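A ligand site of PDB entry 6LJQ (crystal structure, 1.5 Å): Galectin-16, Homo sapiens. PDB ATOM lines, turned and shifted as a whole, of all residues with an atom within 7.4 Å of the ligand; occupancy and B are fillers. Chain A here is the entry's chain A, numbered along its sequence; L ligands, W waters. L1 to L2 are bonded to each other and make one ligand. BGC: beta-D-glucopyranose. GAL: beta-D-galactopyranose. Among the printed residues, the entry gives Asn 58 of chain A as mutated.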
ATOM      1  N   PRO A  37      -7.764 -13.161  22.537  1.00  0.00           N
ATOM      2  CA  PRO A  37      -8.318 -13.314  23.898  1.00  0.00           C
ATOM      3  C   PRO A  37      -9.839 -13.424  23.893  1.00  0.00           C
ATOM      4  O   PRO A  37     -10.519 -12.977  22.968  1.00  0.00           O
ATOM      5  CB  PRO A  37      -7.851 -12.036  24.615  1.00  0.00           C
ATOM      6  CG  PRO A  37      -7.570 -11.060  23.522  1.00  0.00           C
ATOM      7  CD  PRO A  37      -7.118 -11.858  22.338  1.00  0.00           C
ATOM      8  N   GLN A  40     -11.354  -8.609  26.585  1.00  0.00           N
ATOM      9  CA  GLN A  40     -10.396  -7.522  26.648  1.00  0.00           C
ATOM     10  C   GLN A  40     -11.046  -6.311  27.285  1.00  0.00           C
ATOM     11  O   GLN A  40     -12.197  -5.992  26.979  1.00  0.00           O
ATOM     12  CB  GLN A  40      -9.870  -7.155  25.259  1.00  0.00           C
ATOM     13  CG  GLN A  40      -8.711  -6.166  25.305  1.00  0.00           C
ATOM     14  CD  GLN A  40      -7.940  -6.125  23.998  1.00  0.00           C
ATOM     15  OE1 GLN A  40      -7.794  -7.144  23.327  1.00  0.00           O
ATOM     16  NE2 GLN A  40      -7.451  -4.938  23.633  1.00  0.00           N
ATOM     17  N   ASP A  42      -9.978  -2.230  28.144  1.00  0.00           N
ATOM     18  CA  ASP A  42      -9.004  -1.154  27.973  1.00  0.00           C
ATOM     19  C   ASP A  42      -9.533   0.130  28.604  1.00  0.00           C
ATOM     20  O   ASP A  42     -10.705   0.472  28.422  1.00  0.00           O
ATOM     21  CB  ASP A  42      -8.706  -0.913  26.497  1.00  0.00           C
ATOM     22  CG  ASP A  42      -8.022  -2.085  25.842  1.00  0.00           C
ATOM     23  OD1 ASP A  42      -6.862  -2.387  26.190  1.00  0.00           O
ATOM     24  OD2 ASP A  42      -8.645  -2.699  24.957  1.00  0.00           O
ATOM     25  N   HIS A  56      -4.837  -2.188  30.522  1.00  0.00           N
ATOM     26  CA  HIS A  56      -5.285  -3.117  29.511  1.00  0.00           C
ATOM     27  C   HIS A  56      -5.255  -4.484  30.172  1.00  0.00           C
ATOM     28  O   HIS A  56      -4.269  -4.836  30.808  1.00  0.00           O
ATOM     29  CB  HIS A  56      -4.335  -3.081  28.320  1.00  0.00           C
ATOM     30  CG  HIS A  56      -4.398  -4.286  27.445  1.00  0.00           C
ATOM     31  ND1 HIS A  56      -5.304  -4.412  26.417  1.00  0.00           N
ATOM     32  CD2 HIS A  56      -3.639  -5.406  27.424  1.00  0.00           C
ATOM     33  CE1 HIS A  56      -5.124  -5.583  25.816  1.00  0.00           C
ATOM     34  NE2 HIS A  56      -4.119  -6.200  26.409  1.00  0.00           N
ATOM     35  N   LEU A  57      -6.335  -5.232  30.036  1.00  0.00           N
ATOM     36  CA  LEU A  57      -6.417  -6.578  30.561  1.00  0.00           C
ATOM     37  C   LEU A  57      -7.005  -7.480  29.496  1.00  0.00           C
ATOM     38  O   LEU A  57      -8.034  -7.146  28.895  1.00  0.00           O
ATOM     39  CB  LEU A  57      -7.285  -6.631  31.823  1.00  0.00           C
ATOM     40  CG  LEU A  57      -7.497  -7.991  32.498  1.00  0.00           C
ATOM     41  CD1 LEU A  57      -7.601  -7.766  33.982  1.00  0.00           C
ATOM     42  CD2 LEU A  57      -8.743  -8.702  31.983  1.00  0.00           C
ATOM     43  N   ASN A  58      -6.388  -8.636  29.274  1.00  0.00           N
ATOM     44  CA  ASN A  58      -7.035  -9.599  28.403  1.00  0.00           C
ATOM     45  C   ASN A  58      -6.929 -10.988  29.012  1.00  0.00           C
ATOM     46  O   ASN A  58      -6.020 -11.276  29.789  1.00  0.00           O
ATOM     47  CB  ASN A  58      -6.555  -9.551  26.947  1.00  0.00           C
ATOM     48  CG  ASN A  58      -5.196 -10.125  26.770  1.00  0.00           C
ATOM     49  OD1 ASN A  58      -5.009 -11.343  26.831  1.00  0.00           O
ATOM     50  ND2 ASN A  58      -4.209  -9.262  26.536  1.00  0.00           N
ATOM     51  N   HIS A  60      -6.894 -15.123  28.326  1.00  0.00           N
ATOM     52  CA  HIS A  60      -6.732 -16.294  27.473  1.00  0.00           C
ATOM     53  C   HIS A  60      -7.094 -17.486  28.347  1.00  0.00           C
ATOM     54  O   HIS A  60      -6.280 -17.922  29.174  1.00  0.00           O
ATOM     55  CB  HIS A  60      -5.302 -16.407  26.972  1.00  0.00           C
ATOM     56  CG  HIS A  60      -4.948 -15.373  25.960  1.00  0.00           C
ATOM     57  ND1 HIS A  60      -5.217 -15.516  24.624  1.00  0.00           N
ATOM     58  CD2 HIS A  60      -4.371 -14.154  26.107  1.00  0.00           C
ATOM     59  CE1 HIS A  60      -4.806 -14.440  23.971  1.00  0.00           C
ATOM     60  NE2 HIS A  60      -4.287 -13.600  24.858  1.00  0.00           N
ATOM     61  N   ARG A  64      -3.569 -17.619  30.498  1.00  0.00           N
ATOM     62  CA  ARG A  64      -3.019 -16.484  31.206  1.00  0.00           C
ATOM     63  C   ARG A  64      -3.996 -15.325  31.203  1.00  0.00           C
ATOM     64  O   ARG A  64      -4.905 -15.234  30.375  1.00  0.00           O
ATOM     65  CB  ARG A  64      -1.660 -16.056  30.624  1.00  0.00           C
ATOM     66  CG  ARG A  64      -1.749 -15.603  29.168  1.00  0.00           C
ATOM     67  CD  ARG A  64      -0.414 -15.124  28.616  1.00  0.00           C
ATOM     68  NE  ARG A  64      -0.529 -14.779  27.197  1.00  0.00           N
ATOM     69  CZ  ARG A  64       0.187 -13.842  26.593  1.00  0.00           C
ATOM     70  NH1 ARG A  64       1.070 -13.106  27.260  1.00  0.00           N
ATOM     71  NH2 ARG A  64       0.000 -13.615  25.292  1.00  0.00           N
ATOM     72  N   VAL A  66      -3.374 -11.279  30.963  1.00  0.00           N
ATOM     73  CA  VAL A  66      -2.328 -10.365  30.512  1.00  0.00           C
ATOM     74  C   VAL A  66      -2.751  -8.941  30.875  1.00  0.00           C
ATOM     75  O   VAL A  66      -3.892  -8.558  30.625  1.00  0.00           O
ATOM     76  CB  VAL A  66      -2.150 -10.472  28.990  1.00  0.00           C
ATOM     77  CG1 VAL A  66      -0.993  -9.591  28.506  1.00  0.00           C
ATOM     78  CG2 VAL A  66      -1.956 -11.925  28.584  1.00  0.00           C
ATOM     79  N   MET A  67      -1.842  -8.177  31.476  1.00  0.00           N
ATOM     80  CA  MET A  67      -2.083  -6.767  31.748  1.00  0.00           C
ATOM     81  C   MET A  67      -0.935  -5.910  31.230  1.00  0.00           C
ATOM     82  O   MET A  67       0.217  -6.321  31.218  1.00  0.00           O
ATOM     83  CB  MET A  67      -2.333  -6.514  33.232  1.00  0.00           C
ATOM     84  CG  MET A  67      -3.705  -7.013  33.685  1.00  0.00           C
ATOM     85  SD  MET A  67      -3.721  -7.308  35.468  1.00  0.00           S
ATOM     86  CE  MET A  67      -2.685  -8.763  35.497  1.00  0.00           C
ATOM     87  N   ASN A  68      -1.263  -4.704  30.790  1.00  0.00           N
ATOM     88  CA  ASN A  68      -0.226  -3.817  30.275  1.00  0.00           C
ATOM     89  C   ASN A  68      -0.833  -2.426  30.184  1.00  0.00           C
ATOM     90  O   ASN A  68      -2.006  -2.213  30.527  1.00  0.00           O
ATOM     91  CB  ASN A  68       0.281  -4.290  28.913  1.00  0.00           C
ATOM     92  CG  ASN A  68       1.710  -3.885  28.635  1.00  0.00           C
ATOM     93  OD1 ASN A  68       2.242  -2.966  29.260  1.00  0.00           O
ATOM     94  ND2 ASN A  68       2.349  -4.569  27.684  1.00  0.00           N
ATOM     95  N   SER A  69      -0.027  -1.479  29.716  1.00  0.00           N
ATOM     96  CA  SER A  69      -0.493  -0.158  29.325  1.00  0.00           C
ATOM     97  C   SER A  69       0.023   0.096  27.917  1.00  0.00           C
ATOM     98  O   SER A  69       0.957  -0.556  27.454  1.00  0.00           O
ATOM     99  CB  SER A  69       0.074   0.934  30.235  1.00  0.00           C
ATOM    100  OG  SER A  69       1.503   0.852  30.251  1.00  0.00           O
ATOM    101  N   TRP A  75       3.179  -0.630  23.633  1.00  0.00           N
ATOM    102  CA  TRP A  75       2.865  -1.548  24.722  1.00  0.00           C
ATOM    103  C   TRP A  75       4.062  -1.643  25.649  1.00  0.00           C
ATOM    104  O   TRP A  75       5.192  -1.888  25.209  1.00  0.00           O
ATOM    105  CB  TRP A  75       2.494  -2.928  24.175  1.00  0.00           C
ATOM    106  CG  TRP A  75       1.187  -2.907  23.480  1.00  0.00           C
ATOM    107  CD1 TRP A  75       0.961  -3.005  22.145  1.00  0.00           C
ATOM    108  CD2 TRP A  75      -0.091  -2.727  24.090  1.00  0.00           C
ATOM    109  NE1 TRP A  75      -0.379  -2.913  21.880  1.00  0.00           N
ATOM    110  CE2 TRP A  75      -1.058  -2.743  23.072  1.00  0.00           C
ATOM    111  CE3 TRP A  75      -0.520  -2.573  25.420  1.00  0.00           C
ATOM    112  CZ2 TRP A  75      -2.417  -2.605  23.322  1.00  0.00           C
ATOM    113  CZ3 TRP A  75      -1.870  -2.439  25.668  1.00  0.00           C
ATOM    114  CH2 TRP A  75      -2.805  -2.447  24.633  1.00  0.00           C
ATOM    115  N   MET A  76       3.816  -1.435  26.947  1.00  0.00           N
ATOM    116  CA  MET A  76       4.902  -1.320  27.915  1.00  0.00           C
ATOM    117  C   MET A  76       5.202  -2.675  28.555  1.00  0.00           C
ATOM    118  O   MET A  76       5.114  -3.709  27.879  1.00  0.00           O
ATOM    119  CB  MET A  76       4.576  -0.218  28.921  1.00  0.00           C
ATOM    120  CG  MET A  76       4.326   1.144  28.252  1.00  0.00           C
ATOM    121  SD  MET A  76       5.783   1.799  27.397  1.00  0.00           S
ATOM    122  CE  MET A  76       6.752   2.395  28.784  1.00  0.00           C
ATOM    123  N   LEU A  77       5.554  -2.695  29.837  1.00  0.00           N
ATOM    124  CA  LEU A  77       5.967  -3.954  30.451  1.00  0.00           C
ATOM    125  C   LEU A  77       4.751  -4.848  30.679  1.00  0.00           C
ATOM    126  O   LEU A  77       3.844  -4.493  31.444  1.00  0.00           O
ATOM    127  CB  LEU A  77       6.683  -3.679  31.765  1.00  0.00           C
ATOM    128  CG  LEU A  77       8.004  -2.913  31.578  1.00  0.00           C
ATOM    129  CD1 LEU A  77       8.591  -2.447  32.902  1.00  0.00           C
ATOM    130  CD2 LEU A  77       9.003  -3.781  30.815  1.00  0.00           C
ATOM    131  N   GLU A  78       4.719  -5.995  30.016  1.00  0.00           N
ATOM    132  CA  GLU A  78       3.607  -6.914  30.140  1.00  0.00           C
ATOM    133  C   GLU A  78       3.704  -7.636  31.483  1.00  0.00           C
ATOM    134  O   GLU A  78       4.778  -8.073  31.893  1.00  0.00           O
ATOM    135  CB  GLU A  78       3.660  -7.936  29.009  1.00  0.00           C
ATOM    136  CG  GLU A  78       2.399  -8.737  28.838  1.00  0.00           C
ATOM    137  CD  GLU A  78       2.465  -9.595  27.586  1.00  0.00           C
ATOM    138  OE1 GLU A  78       2.937 -10.748  27.673  1.00  0.00           O
ATOM    139  OE2 GLU A  78       2.038  -9.107  26.503  1.00  0.00           O
ATOM    140  N   GLU A  79       2.548  -7.730  32.145  1.00  0.00           N
ATOM    141  CA  GLU A  79       2.414  -8.434  33.446  1.00  0.00           C
ATOM    142  C   GLU A  79       1.536  -9.655  33.168  1.00  0.00           C
ATOM    143  O   GLU A  79       0.400  -9.473  32.732  1.00  0.00           O
ATOM    144  CB  GLU A  79       1.787  -7.479  34.460  1.00  0.00           C
ATOM    145  CG  GLU A  79       2.731  -7.090  35.574  1.00  0.00           C
ATOM    146  CD  GLU A  79       3.519  -5.800  35.414  1.00  0.00           C
ATOM    147  OE1 GLU A  79       3.022  -4.731  35.821  1.00  0.00           O
ATOM    148  OE2 GLU A  79       4.650  -5.883  34.929  1.00  0.00           O
ATOM    149  N   ASN A  80       2.040 -10.861  33.437  1.00  0.00           N
ATOM    150  CA  ASN A  80       1.300 -12.067  33.103  1.00  0.00           C
ATOM    151  C   ASN A  80       0.957 -12.837  34.370  1.00  0.00           C
ATOM    152  O   ASN A  80       1.806 -13.020  35.246  1.00  0.00           O
ATOM    153  CB  ASN A  80       2.083 -12.976  32.168  1.00  0.00           C
ATOM    154  CG  ASN A  80       2.199 -12.406  30.776  1.00  0.00           C
ATOM    155  OD1 ASN A  80       1.224 -12.411  30.019  1.00  0.00           O
ATOM    156  ND2 ASN A  80       3.380 -11.908  30.439  1.00  0.00           N
ATOM    157  N   TRP A 130     -14.510  -5.701  25.286  1.00  0.00           N
ATOM    158  CA  TRP A 130     -14.780  -6.327  24.008  1.00  0.00           C
ATOM    159  C   TRP A 130     -14.206  -7.734  23.976  1.00  0.00           C
ATOM    160  O   TRP A 130     -13.863  -8.308  25.017  1.00  0.00           O
ATOM    161  CB  TRP A 130     -14.344  -5.420  22.853  1.00  0.00           C
ATOM    162  CG  TRP A 130     -12.863  -5.095  22.789  1.00  0.00           C
ATOM    163  CD1 TRP A 130     -12.122  -4.417  23.712  1.00  0.00           C
ATOM    164  CD2 TRP A 130     -11.976  -5.411  21.712  1.00  0.00           C
ATOM    165  NE1 TRP A 130     -10.815  -4.295  23.286  1.00  0.00           N
ATOM    166  CE2 TRP A 130     -10.701  -4.908  22.063  1.00  0.00           C
ATOM    167  CE3 TRP A 130     -12.125  -6.079  20.487  1.00  0.00           C
ATOM    168  CZ2 TRP A 130      -9.592  -5.032  21.223  1.00  0.00           C
ATOM    169  CZ3 TRP A 130     -11.017  -6.216  19.662  1.00  0.00           C
ATOM    170  CH2 TRP A 130      -9.768  -5.691  20.043  1.00  0.00           C
ATOM    171  N   ARG A 131     -14.093  -8.277  22.761  1.00  0.00           N
ATOM    172  CA  ARG A 131     -13.945  -9.698  22.457  1.00  0.00           C
ATOM    173  C   ARG A 131     -15.281 -10.403  22.655  1.00  0.00           C
ATOM    174  O   ARG A 131     -16.299  -9.752  22.952  1.00  0.00           O
ATOM    175  CB  ARG A 131     -12.796 -10.361  23.221  1.00  0.00           C
ATOM    176  CG  ARG A 131     -11.478  -9.583  23.124  1.00  0.00           C
ATOM    177  CD  ARG A 131     -10.956  -9.487  21.699  1.00  0.00           C
ATOM    178  NE  ARG A 131      -9.651  -8.834  21.665  1.00  0.00           N
ATOM    179  CZ  ARG A 131      -8.863  -8.817  20.604  1.00  0.00           C
ATOM    180  NH1 ARG A 131      -9.245  -9.418  19.485  1.00  0.00           N
ATOM    181  NH2 ARG A 131      -7.688  -8.186  20.660  1.00  0.00           N
HETATM  182  C2  BGC L   1       3.066 -11.656  23.826  1.00  0.00           C
HETATM  183  C3  BGC L   1       1.707 -11.045  23.531  1.00  0.00           C
HETATM  184  C4  BGC L   1       1.848  -9.729  22.759  1.00  0.00           C
HETATM  185  C5  BGC L   1       2.832  -9.887  21.588  1.00  0.00           C
HETATM  186  C6  BGC L   1       3.220  -8.532  21.016  1.00  0.00           C
HETATM  187  C1  BGC L   1       3.796 -11.799  22.501  1.00  0.00           C
HETATM  188  O1  BGC L   1       5.022 -12.441  22.733  1.00  0.00           O
HETATM  189  O2  BGC L   1       2.912 -12.910  24.424  1.00  0.00           O
HETATM  190  O3  BGC L   1       1.042 -10.833  24.747  1.00  0.00           O
HETATM  191  O4  BGC L   1       0.589  -9.367  22.257  1.00  0.00           O
HETATM  192  O5  BGC L   1       4.030 -10.528  21.990  1.00  0.00           O
HETATM  193  O6  BGC L   1       3.368  -8.618  19.629  1.00  0.00           O
HETATM  194  C1  GAL L   2       0.193  -8.058  22.576  1.00  0.00           C
HETATM  195  C2  GAL L   2      -1.136  -7.776  21.880  1.00  0.00           C
HETATM  196  C3  GAL L   2      -1.667  -6.408  22.305  1.00  0.00           C
HETATM  197  C4  GAL L   2      -1.725  -6.394  23.835  1.00  0.00           C
HETATM  198  C5  GAL L   2      -0.306  -6.622  24.334  1.00  0.00           C
HETATM  199  C6  GAL L   2      -0.259  -6.491  25.855  1.00  0.00           C
HETATM  200  O2  GAL L   2      -0.968  -7.816  20.494  1.00  0.00           O
HETATM  201  O3  GAL L   2      -2.937  -6.193  21.754  1.00  0.00           O
HETATM  202  O4  GAL L   2      -2.550  -7.430  24.331  1.00  0.00           O
HETATM  203  O5  GAL L   2       0.083  -7.917  23.974  1.00  0.00           O
HETATM  204  O6  GAL L   2       1.061  -6.670  26.295  1.00  0.00           O
HETATM  205  O   HOH W   1      -0.611 -10.450  19.596  1.00  0.00           O
HETATM  206  O   HOH W   2      -5.157  -8.356  23.019  1.00  0.00           O
HETATM  207  O   HOH W   3      -1.676 -10.120  24.909  1.00  0.00           O
HETATM  208  O   HOH W   4      -5.306  -4.864  21.576  1.00  0.00           O
HETATM  209  O   HOH W   5       6.108 -15.084  23.381  1.00  0.00           O
HETATM  210  O   HOH W   6       3.430  -6.461  24.638  1.00  0.00           O
HETATM  211  O   HOH W   7       5.141 -14.224  25.743  1.00  0.00           O
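The side-chain carboxylate (OE2) of Glu 78 lies within hydrogen-bond range of an oxygen (O6) of GAL L2, at 2.6 Å.
The side-chain amide nitrogen (ND2) of Asn 68 lies within hydrogen-bond range of an oxygen (O6) of GAL L2 (2.8 Å).
NE2 of His 56 is in hydrogen-bond range of O4 of GAL L2 (2.9 Å).
The guanidinium group (NH2) of Arg 64 lies within hydrogen-bond range of an oxygen (O3) of BGC L1.
The side-chain amide nitrogen (ND2) of Asn 58 sits at hydrogen-bond distance from an oxygen (O4) of GAL L2, at 3.3 Å.
The side-chain carboxylate of Glu 78 lies within salt-bridge range of the guanidinium group of Arg 64.
OE1 of Glu 78 sits at hydrogen-bond distance from ND2 of Asn 80 (3.0 Å).
The backbone carbonyl oxygen (O) of Asn 68 is in hydrogen-bond range of the backbone NH (N) of His 56 (2.8 Å).
ND2 of Asn 68 lies within hydrogen-bond range of O of Met 76.
The side-chain amide oxygen (OD1) of Asn 68 sits close to the backbone carbonyl oxygen (O) of Leu 77 (3.1 Å).
The side-chain carboxylate of Asp 42 lies within hydrogen-bond range of a ring nitrogen (ND1) of His 56 (2.6 Å).
The guanidinium group (NH1) of Arg 64 sits at hydrogen-bond distance from the side-chain amide oxygen (OD1) of Asn 80, at 2.8 Å.
The backbone NH (N) of Asn 58 is in hydrogen-bond range of the backbone carbonyl oxygen (O) of Val 66, 2.8 Å away.
NE1 of Trp 75 touches C3 of GAL L2, 3.7 Å away.
Hydrophobic or aromatic side chains within 4 Å of the ligand: His 56 and Trp 75.
Within 4 Å of the ligand: His 56, Asn 58, Arg 64, Asn 68, Trp 75 and Glu 78.
The nearest printed residue that does not touch the ligand is Val 66 (4.1 Å).
Water W4 bridges O3 of GAL L2 (2.7 Å) and NE2 of Gln 40 (3.0 Å).
Water W3 bridges O3 of BGC L1 (2.8 Å) and ND2 of Asn 58 (3.1 Å).
Water W2 lies within hydrogen-bond range of the side-chain amide oxygen (OE1) of Gln 40, an oxygen (O4) of GAL L2 and the guanidinium group (NH2) of Arg 131.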
